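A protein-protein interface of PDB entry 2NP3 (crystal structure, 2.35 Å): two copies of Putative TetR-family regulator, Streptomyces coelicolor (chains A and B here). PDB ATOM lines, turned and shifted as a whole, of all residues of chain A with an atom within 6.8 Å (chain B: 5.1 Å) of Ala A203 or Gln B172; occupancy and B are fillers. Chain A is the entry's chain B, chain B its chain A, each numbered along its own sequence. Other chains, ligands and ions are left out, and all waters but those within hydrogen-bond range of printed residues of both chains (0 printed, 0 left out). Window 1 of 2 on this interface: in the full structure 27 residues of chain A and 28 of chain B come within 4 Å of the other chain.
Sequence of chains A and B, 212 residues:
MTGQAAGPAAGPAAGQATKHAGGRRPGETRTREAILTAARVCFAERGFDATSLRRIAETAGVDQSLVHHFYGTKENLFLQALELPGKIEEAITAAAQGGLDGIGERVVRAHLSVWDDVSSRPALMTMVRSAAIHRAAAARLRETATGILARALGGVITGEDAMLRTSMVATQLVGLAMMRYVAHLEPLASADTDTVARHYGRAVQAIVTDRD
The side-chain amide nitrogen (NE2) of Gln B172 lies within hydrogen-bond range of the side-chain amide oxygen (OE1) of Gln A172, 3.2 Å away.
OH of Tyr B200 sits at hydrogen-bond distance from O of Gln B172, 2.8 Å away.
The side-chain amide nitrogen (NE2) of Gln B172 lies within hydrogen-bond range of the backbone carbonyl oxygen (O) of Ala B203 (3.4 Å).
O of Gln A172 lies within hydrogen-bond range of OH of Tyr A200 (2.7 Å).
The side-chain amide oxygen (OE1) of Gln B172 sits close to the backbone carbonyl oxygen (O) of Met B168 (3.2 Å).
CG2 of Thr A171 touches C of Gly B175, at 3.6 Å.
Leu B176 touches Thr A171.
Thr A171 touches Tyr B200.
OH of Tyr B200 touches CG of Gln A172, 3.8 Å away.
Gly A175 touches Thr B171.
Leu A176 touches Thr B171 (N to CG2, 3.7 Å).
CD1 of Ile B207 touches O of His A199, 3.4 Å away.
O of Ala A203 touches CB of Ala B203 (3.7 Å).
Ala A206 touches Ala B206 (CB to CB, 3.9 Å).
Ala B203 touches Ile A207.
Ala A203 touches just these residues of chain B: Gln B172, Ala B203 and Ile B207.
Of chain A, only Gln A172, Tyr A200 and Ala A203 come within 4 Å of Gln B172.
Of the printed residues of chain B, Thr A171 touches Gly B175 (3.6 Å), Leu B176 (3.8 Å) and Tyr B200 (3.9 Å).
Printed residues of chain B within 4 Å of Met A179: Thr B171 and Val B174.
Of the printed residues of chain B, Arg A202 touches Ala B206 (3.6 Å).
Val B169 touches none of the printed residues of chain A.
Of the 14 printed residues of chain B, 10 touch a printed residue of chain A.
Hydrophobic or aromatic side chains of chain A that line the printed part of chain B: Met A179, His A199, Tyr A200, Ala A203, Ala A206 and Ile A207.
Among the printed residues, 20 pairs touch across the chains.
Among the printed residues, no Asp or Glu carboxylate lies within 4 Å of a Lys or Arg side-chain nitrogen of the other chain.
Thr A171 touches Gly B175, and with the chains exchanged Gly A175 touches Thr B171.
Gln B172 touches its own counterpart, Gln A172.
Gln A172 touches Tyr B200, and with the chains exchanged Tyr A200 touches Gln B172.
Ala A203 touches Ile B207, and with the chains exchanged Ile A207 touches Ala B203.
Of the 20 pairs that touch across the chains among the printed residues, 13 have their exchanged pair printed and touching as well.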
ATOM      1  N   GLY A 104      -3.061  -1.568  27.757  1.00  0.00           N
ATOM      2  CA  GLY A 104      -3.977  -1.958  26.730  1.00  0.00           C
ATOM      3  C   GLY A 104      -5.442  -1.818  27.157  1.00  0.00           C
ATOM      4  O   GLY A 104      -6.212  -1.139  26.496  1.00  0.00           O
ATOM      5  N   VAL A 169      -2.207   0.256  17.094  1.00  0.00           N
ATOM      6  CA  VAL A 169      -3.143   0.510  18.208  1.00  0.00           C
ATOM      7  C   VAL A 169      -4.264   1.467  17.798  1.00  0.00           C
ATOM      8  O   VAL A 169      -5.435   1.208  18.117  1.00  0.00           O
ATOM      9  CB  VAL A 169      -2.421   1.078  19.448  1.00  0.00           C
ATOM     10  CG1 VAL A 169      -3.421   1.542  20.504  1.00  0.00           C
ATOM     11  CG2 VAL A 169      -1.403   0.054  20.014  1.00  0.00           C
ATOM     12  N   THR A 171      -5.424   2.087  14.713  1.00  0.00           N
ATOM     13  CA  THR A 171      -6.254   1.289  13.829  1.00  0.00           C
ATOM     14  C   THR A 171      -7.227   0.370  14.579  1.00  0.00           C
ATOM     15  O   THR A 171      -8.386   0.325  14.246  1.00  0.00           O
ATOM     16  CB  THR A 171      -5.310   0.455  12.992  1.00  0.00           C
ATOM     17  OG1 THR A 171      -4.575   1.358  12.173  1.00  0.00           O
ATOM     18  CG2 THR A 171      -6.029  -0.479  12.122  1.00  0.00           C
ATOM     19  N   GLN A 172      -6.719  -0.370  15.562  1.00  0.00           N
ATOM     20  CA  GLN A 172      -7.533  -1.207  16.429  1.00  0.00           C
ATOM     21  C   GLN A 172      -8.682  -0.497  17.142  1.00  0.00           C
ATOM     22  O   GLN A 172      -9.771  -1.015  17.249  1.00  0.00           O
ATOM     23  CB  GLN A 172      -6.626  -1.899  17.465  1.00  0.00           C
ATOM     24  CG  GLN A 172      -5.778  -3.031  16.861  1.00  0.00           C
ATOM     25  CD  GLN A 172      -4.801  -3.680  17.883  1.00  0.00           C
ATOM     26  OE1 GLN A 172      -4.816  -4.892  18.073  1.00  0.00           O
ATOM     27  NE2 GLN A 172      -3.983  -2.870  18.541  1.00  0.00           N
ATOM     28  N   GLY A 175     -11.182   0.763  14.517  1.00  0.00           N
ATOM     29  CA  GLY A 175     -11.906  -0.373  13.993  1.00  0.00           C
ATOM     30  C   GLY A 175     -12.914  -0.828  15.017  1.00  0.00           C
ATOM     31  O   GLY A 175     -14.025  -1.140  14.645  1.00  0.00           O
ATOM     32  N   LEU A 176     -12.537  -0.864  16.313  1.00  0.00           N
ATOM     33  CA  LEU A 176     -13.489  -1.233  17.381  1.00  0.00           C
ATOM     34  C   LEU A 176     -14.675  -0.276  17.446  1.00  0.00           C
ATOM     35  O   LEU A 176     -15.833  -0.726  17.559  1.00  0.00           O
ATOM     36  CB  LEU A 176     -12.780  -1.273  18.737  1.00  0.00           C
ATOM     37  CG  LEU A 176     -13.558  -1.475  20.027  1.00  0.00           C
ATOM     38  CD1 LEU A 176     -14.330  -2.784  20.005  1.00  0.00           C
ATOM     39  CD2 LEU A 176     -12.638  -1.359  21.291  1.00  0.00           C
ATOM     40  N   MET A 179     -17.188  -0.722  14.461  1.00  0.00           N
ATOM     41  CA  MET A 179     -17.986  -1.933  14.454  1.00  0.00           C
ATOM     42  C   MET A 179     -18.938  -2.027  15.625  1.00  0.00           C
ATOM     43  O   MET A 179     -19.974  -2.568  15.488  1.00  0.00           O
ATOM     44  CB  MET A 179     -17.074  -3.180  14.450  1.00  0.00           C
ATOM     45  CG  MET A 179     -16.191  -3.324  13.247  1.00  0.00           C
ATOM     46  SD  MET A 179     -17.180  -3.497  11.546  1.00  0.00           S
ATOM     47  CE  MET A 179     -15.473  -3.409  10.359  1.00  0.00           C
ATOM     48  N   ARG A 198     -11.773  -6.176  28.493  1.00  0.00           N
ATOM     49  CA  ARG A 198     -10.944  -7.260  28.898  1.00  0.00           C
ATOM     50  C   ARG A 198     -10.401  -7.995  27.711  1.00  0.00           C
ATOM     51  O   ARG A 198      -9.201  -8.199  27.650  1.00  0.00           O
ATOM     52  CB  ARG A 198     -11.663  -8.225  29.878  1.00  0.00           C
ATOM     53  N   HIS A 199     -11.243  -8.378  26.745  1.00  0.00           N
ATOM     54  CA  HIS A 199     -10.716  -9.101  25.561  1.00  0.00           C
ATOM     55  C   HIS A 199      -9.949  -8.254  24.543  1.00  0.00           C
ATOM     56  O   HIS A 199      -8.920  -8.667  24.041  1.00  0.00           O
ATOM     57  CB  HIS A 199     -11.807  -9.877  24.826  1.00  0.00           C
ATOM     58  CG  HIS A 199     -12.425 -10.969  25.639  1.00  0.00           C
ATOM     59  ND1 HIS A 199     -11.877 -12.224  25.735  1.00  0.00           N
ATOM     60  CD2 HIS A 199     -13.561 -11.000  26.369  1.00  0.00           C
ATOM     61  CE1 HIS A 199     -12.634 -12.976  26.507  1.00  0.00           C
ATOM     62  NE2 HIS A 199     -13.661 -12.253  26.907  1.00  0.00           N
ATOM     63  N   TYR A 200     -10.453  -7.097  24.196  1.00  0.00           N
ATOM     64  CA  TYR A 200      -9.767  -6.299  23.197  1.00  0.00           C
ATOM     65  C   TYR A 200      -8.508  -5.670  23.818  1.00  0.00           C
ATOM     66  O   TYR A 200      -7.513  -5.529  23.142  1.00  0.00           O
ATOM     67  CB  TYR A 200     -10.708  -5.273  22.584  1.00  0.00           C
ATOM     68  CG  TYR A 200     -10.402  -4.861  21.127  1.00  0.00           C
ATOM     69  CD1 TYR A 200     -10.659  -5.736  20.065  1.00  0.00           C
ATOM     70  CD2 TYR A 200      -9.874  -3.613  20.832  1.00  0.00           C
ATOM     71  CE1 TYR A 200     -10.468  -5.338  18.738  1.00  0.00           C
ATOM     72  CE2 TYR A 200      -9.700  -3.193  19.532  1.00  0.00           C
ATOM     73  CZ  TYR A 200      -9.967  -4.080  18.473  1.00  0.00           C
ATOM     74  OH  TYR A 200      -9.758  -3.717  17.165  1.00  0.00           O
ATOM     75  N   GLY A 201      -8.519  -5.399  25.119  1.00  0.00           N
ATOM     76  CA  GLY A 201      -7.302  -4.987  25.832  1.00  0.00           C
ATOM     77  C   GLY A 201      -6.039  -5.788  25.578  1.00  0.00           C
ATOM     78  O   GLY A 201      -4.944  -5.224  25.452  1.00  0.00           O
ATOM     79  N   ARG A 202      -6.192  -7.107  25.530  1.00  0.00           N
ATOM     80  CA  ARG A 202      -5.110  -8.061  25.248  1.00  0.00           C
ATOM     81  C   ARG A 202      -4.505  -7.838  23.903  1.00  0.00           C
ATOM     82  O   ARG A 202      -3.272  -7.932  23.733  1.00  0.00           O
ATOM     83  CB  ARG A 202      -5.633  -9.518  25.307  1.00  0.00           C
ATOM     84  CG  ARG A 202      -5.767 -10.018  26.757  1.00  0.00           C
ATOM     85  CD  ARG A 202      -6.915 -10.956  26.972  1.00  0.00           C
ATOM     86  N   ALA A 203      -5.362  -7.549  22.934  1.00  0.00           N
ATOM     87  CA  ALA A 203      -4.919  -7.284  21.590  1.00  0.00           C
ATOM     88  C   ALA A 203      -4.005  -6.037  21.581  1.00  0.00           C
ATOM     89  O   ALA A 203      -2.999  -6.010  20.911  1.00  0.00           O
ATOM     90  CB  ALA A 203      -6.112  -7.104  20.688  1.00  0.00           C
ATOM     91  N   VAL A 204      -4.354  -5.024  22.366  1.00  0.00           N
ATOM     92  CA  VAL A 204      -3.631  -3.754  22.408  1.00  0.00           C
ATOM     93  C   VAL A 204      -2.374  -3.934  23.267  1.00  0.00           C
ATOM     94  O   VAL A 204      -1.288  -3.564  22.862  1.00  0.00           O
ATOM     95  CB  VAL A 204      -4.516  -2.654  22.992  1.00  0.00           C
ATOM     96  CG1 VAL A 204      -3.700  -1.366  23.205  1.00  0.00           C
ATOM     97  CG2 VAL A 204      -5.773  -2.395  22.124  1.00  0.00           C
ATOM     98  N   GLN A 205      -2.539  -4.532  24.450  1.00  0.00           N
ATOM     99  CA  GLN A 205      -1.402  -4.976  25.294  1.00  0.00           C
ATOM    100  C   GLN A 205      -0.307  -5.693  24.535  1.00  0.00           C
ATOM    101  O   GLN A 205       0.861  -5.468  24.781  1.00  0.00           O
ATOM    102  CB  GLN A 205      -1.881  -5.894  26.430  1.00  0.00           C
ATOM    103  CG  GLN A 205      -0.934  -5.994  27.570  1.00  0.00           C
ATOM    104  CD  GLN A 205      -0.623  -4.620  28.120  1.00  0.00           C
ATOM    105  OE1 GLN A 205      -1.516  -3.808  28.241  1.00  0.00           O
ATOM    106  NE2 GLN A 205       0.653  -4.340  28.421  1.00  0.00           N
ATOM    107  N   ALA A 206      -0.694  -6.544  23.596  1.00  0.00           N
ATOM    108  CA  ALA A 206       0.256  -7.310  22.803  1.00  0.00           C
ATOM    109  C   ALA A 206       1.143  -6.435  21.821  1.00  0.00           C
ATOM    110  O   ALA A 206       2.328  -6.747  21.602  1.00  0.00           O
ATOM    111  CB  ALA A 206      -0.442  -8.466  22.118  1.00  0.00           C
ATOM    112  N   ILE A 207       0.589  -5.353  21.281  1.00  0.00           N
ATOM    113  CA  ILE A 207       1.377  -4.402  20.498  1.00  0.00           C
ATOM    114  C   ILE A 207       2.298  -3.601  21.440  1.00  0.00           C
ATOM    115  O   ILE A 207       3.481  -3.421  21.134  1.00  0.00           O
ATOM    116  CB  ILE A 207       0.529  -3.397  19.676  1.00  0.00           C
ATOM    117  CG1 ILE A 207      -0.556  -4.068  18.811  1.00  0.00           C
ATOM    118  CG2 ILE A 207       1.413  -2.543  18.763  1.00  0.00           C
ATOM    119  CD1 ILE A 207      -0.052  -4.774  17.599  1.00  0.00           C
ATOM    120  N   VAL A 208       1.756  -3.146  22.583  1.00  0.00           N
ATOM    121  CA  VAL A 208       2.537  -2.467  23.633  1.00  0.00           C
ATOM    122  C   VAL A 208       3.730  -3.268  24.123  1.00  0.00           C
ATOM    123  O   VAL A 208       4.814  -2.737  24.176  1.00  0.00           O
ATOM    124  CB  VAL A 208       1.675  -2.041  24.871  1.00  0.00           C
ATOM    125  CG1 VAL A 208       2.578  -1.436  25.975  1.00  0.00           C
ATOM    126  CG2 VAL A 208       0.594  -1.057  24.480  1.00  0.00           C
ATOM    127  N   MET B 168     -13.938  -9.690  16.826  1.00  0.00           N
ATOM    128  CA  MET B 168     -12.736  -8.879  17.034  1.00  0.00           C
ATOM    129  C   MET B 168     -11.590  -9.207  16.088  1.00  0.00           C
ATOM    130  O   MET B 168     -10.856  -8.317  15.717  1.00  0.00           O
ATOM    131  CB  MET B 168     -12.206  -9.044  18.458  1.00  0.00           C
ATOM    132  CG  MET B 168     -13.206  -8.511  19.540  1.00  0.00           C
ATOM    133  SD  MET B 168     -12.657  -8.971  21.363  1.00  0.00           S
ATOM    134  CE  MET B 168     -13.892  -7.944  22.203  1.00  0.00           C
ATOM    135  N   VAL B 169     -11.390 -10.464  15.710  1.00  0.00           N
ATOM    136  CA  VAL B 169     -10.357 -10.744  14.723  1.00  0.00           C
ATOM    137  C   VAL B 169     -10.790 -10.137  13.350  1.00  0.00           C
ATOM    138  O   VAL B 169      -9.999  -9.472  12.673  1.00  0.00           O
ATOM    139  CB  VAL B 169     -10.021 -12.271  14.604  1.00  0.00           C
ATOM    140  CG1 VAL B 169      -9.106 -12.485  13.397  1.00  0.00           C
ATOM    141  CG2 VAL B 169      -9.356 -12.820  15.879  1.00  0.00           C
ATOM    142  N   ALA B 170     -12.029 -10.399  12.943  1.00  0.00           N
ATOM    143  CA  ALA B 170     -12.632  -9.765  11.765  1.00  0.00           C
ATOM    144  C   ALA B 170     -12.509  -8.240  11.794  1.00  0.00           C
ATOM    145  O   ALA B 170     -12.104  -7.656  10.788  1.00  0.00           O
ATOM    146  CB  ALA B 170     -14.115 -10.162  11.621  1.00  0.00           C
ATOM    147  N   THR B 171     -12.896  -7.598  12.906  1.00  0.00           N
ATOM    148  CA  THR B 171     -12.742  -6.151  13.077  1.00  0.00           C
ATOM    149  C   THR B 171     -11.261  -5.721  12.847  1.00  0.00           C
ATOM    150  O   THR B 171     -11.019  -4.724  12.136  1.00  0.00           O
ATOM    151  CB  THR B 171     -13.223  -5.765  14.471  1.00  0.00           C
ATOM    152  OG1 THR B 171     -14.609  -6.019  14.497  1.00  0.00           O
ATOM    153  CG2 THR B 171     -12.992  -4.250  14.849  1.00  0.00           C
ATOM    154  N   GLN B 172     -10.295  -6.464  13.431  1.00  0.00           N
ATOM    155  CA  GLN B 172      -8.897  -6.083  13.312  1.00  0.00           C
ATOM    156  C   GLN B 172      -8.394  -6.211  11.878  1.00  0.00           C
ATOM    157  O   GLN B 172      -7.607  -5.409  11.455  1.00  0.00           O
ATOM    158  CB  GLN B 172      -7.980  -6.866  14.253  1.00  0.00           C
ATOM    159  CG  GLN B 172      -8.286  -6.794  15.759  1.00  0.00           C
ATOM    160  CD  GLN B 172      -7.518  -7.872  16.522  1.00  0.00           C
ATOM    161  OE1 GLN B 172      -7.828  -9.067  16.415  1.00  0.00           O
ATOM    162  NE2 GLN B 172      -6.498  -7.464  17.273  1.00  0.00           N
ATOM    163  N   LEU B 173      -8.883  -7.195  11.125  1.00  0.00           N
ATOM    164  CA  LEU B 173      -8.420  -7.423   9.763  1.00  0.00           C
ATOM    165  C   LEU B 173      -8.977  -6.397   8.793  1.00  0.00           C
ATOM    166  O   LEU B 173      -8.251  -5.841   7.982  1.00  0.00           O
ATOM    167  CB  LEU B 173      -8.712  -8.844   9.333  1.00  0.00           C
ATOM    168  CG  LEU B 173      -7.968 -10.022  10.017  1.00  0.00           C
ATOM    169  CD1 LEU B 173      -8.524 -11.465   9.575  1.00  0.00           C
ATOM    170  CD2 LEU B 173      -6.385  -9.953   9.968  1.00  0.00           C
ATOM    171  N   VAL B 174     -10.257  -6.074   8.932  1.00  0.00           N
ATOM    172  CA  VAL B 174     -10.856  -4.984   8.202  1.00  0.00           C
ATOM    173  C   VAL B 174     -10.280  -3.595   8.530  1.00  0.00           C
ATOM    174  O   VAL B 174     -10.074  -2.787   7.621  1.00  0.00           O
ATOM    175  CB  VAL B 174     -12.430  -5.003   8.343  1.00  0.00           C
ATOM    176  CG1 VAL B 174     -13.088  -3.869   7.549  1.00  0.00           C
ATOM    177  CG2 VAL B 174     -13.003  -6.387   7.851  1.00  0.00           C
ATOM    178  N   GLY B 175      -9.999  -3.301   9.791  1.00  0.00           N
ATOM    179  CA  GLY B 175      -9.294  -2.062  10.132  1.00  0.00           C
ATOM    180  C   GLY B 175      -7.926  -1.967   9.436  1.00  0.00           C
ATOM    181  O   GLY B 175      -7.590  -0.949   8.816  1.00  0.00           O
ATOM    182  N   LEU B 176      -7.141  -3.039   9.572  1.00  0.00           N
ATOM    183  CA  LEU B 176      -5.827  -3.195   8.928  1.00  0.00           C
ATOM    184  C   LEU B 176      -5.895  -2.789   7.445  1.00  0.00           C
ATOM    185  O   LEU B 176      -5.190  -1.892   7.010  1.00  0.00           O
ATOM    186  CB  LEU B 176      -5.374  -4.655   9.038  1.00  0.00           C
ATOM    187  CG  LEU B 176      -4.061  -5.083   8.369  1.00  0.00           C
ATOM    188  CD1 LEU B 176      -2.896  -4.292   8.887  1.00  0.00           C
ATOM    189  CD2 LEU B 176      -3.796  -6.618   8.478  1.00  0.00           C
ATOM    190  N   TYR B 200       1.343  -6.994  13.882  1.00  0.00           N
ATOM    191  CA  TYR B 200      -0.095  -7.089  13.945  1.00  0.00           C
ATOM    192  C   TYR B 200      -0.555  -8.526  14.163  1.00  0.00           C
ATOM    193  O   TYR B 200      -1.554  -8.730  14.832  1.00  0.00           O
ATOM    194  CB  TYR B 200      -0.693  -6.546  12.661  1.00  0.00           C
ATOM    195  CG  TYR B 200      -2.058  -5.959  12.820  1.00  0.00           C
ATOM    196  CD1 TYR B 200      -2.223  -4.684  13.368  1.00  0.00           C
ATOM    197  CD2 TYR B 200      -3.196  -6.643  12.389  1.00  0.00           C
ATOM    198  CE1 TYR B 200      -3.524  -4.094  13.508  1.00  0.00           C
ATOM    199  CE2 TYR B 200      -4.461  -6.073  12.485  1.00  0.00           C
ATOM    200  CZ  TYR B 200      -4.624  -4.793  13.094  1.00  0.00           C
ATOM    201  OH  TYR B 200      -5.876  -4.179  13.235  1.00  0.00           O
ATOM    202  N   ALA B 203      -1.250  -9.310  17.674  1.00  0.00           N
ATOM    203  CA  ALA B 203      -2.457  -8.718  18.210  1.00  0.00           C
ATOM    204  C   ALA B 203      -3.598  -9.680  17.965  1.00  0.00           C
ATOM    205  O   ALA B 203      -4.530  -9.826  18.782  1.00  0.00           O
ATOM    206  CB  ALA B 203      -2.708  -7.363  17.512  1.00  0.00           C
ATOM    207  N   VAL B 204      -3.522 -10.348  16.835  1.00  0.00           N
ATOM    208  CA  VAL B 204      -4.499 -11.378  16.463  1.00  0.00           C
ATOM    209  C   VAL B 204      -4.288 -12.608  17.307  1.00  0.00           C
ATOM    210  O   VAL B 204      -5.251 -13.273  17.724  1.00  0.00           O
ATOM    211  CB  VAL B 204      -4.432 -11.746  14.938  1.00  0.00           C
ATOM    212  CG1 VAL B 204      -5.411 -12.884  14.603  1.00  0.00           C
ATOM    213  CG2 VAL B 204      -4.749 -10.525  14.088  1.00  0.00           C
ATOM    214  N   ALA B 206      -3.078 -12.825  20.423  1.00  0.00           N
ATOM    215  CA  ALA B 206      -3.689 -12.515  21.734  1.00  0.00           C
ATOM    216  C   ALA B 206      -5.213 -12.707  21.832  1.00  0.00           C
ATOM    217  O   ALA B 206      -5.730 -12.943  22.918  1.00  0.00           O
ATOM    218  CB  ALA B 206      -3.353 -11.104  22.136  1.00  0.00           C
ATOM    219  N   ILE B 207      -5.932 -12.548  20.711  1.00  0.00           N
ATOM    220  CA  ILE B 207      -7.390 -12.699  20.699  1.00  0.00           C
ATOM    221  C   ILE B 207      -7.656 -14.205  20.603  1.00  0.00           C
ATOM    222  O   ILE B 207      -8.464 -14.788  21.364  1.00  0.00           O
ATOM    223  CB  ILE B 207      -8.082 -11.980  19.524  1.00  0.00           C
ATOM    224  CG1 ILE B 207      -7.984 -10.439  19.599  1.00  0.00           C
ATOM    225  CG2 ILE B 207      -9.570 -12.396  19.435  1.00  0.00           C
ATOM    226  CD1 ILE B 207      -8.444  -9.829  20.890  1.00  0.00           C
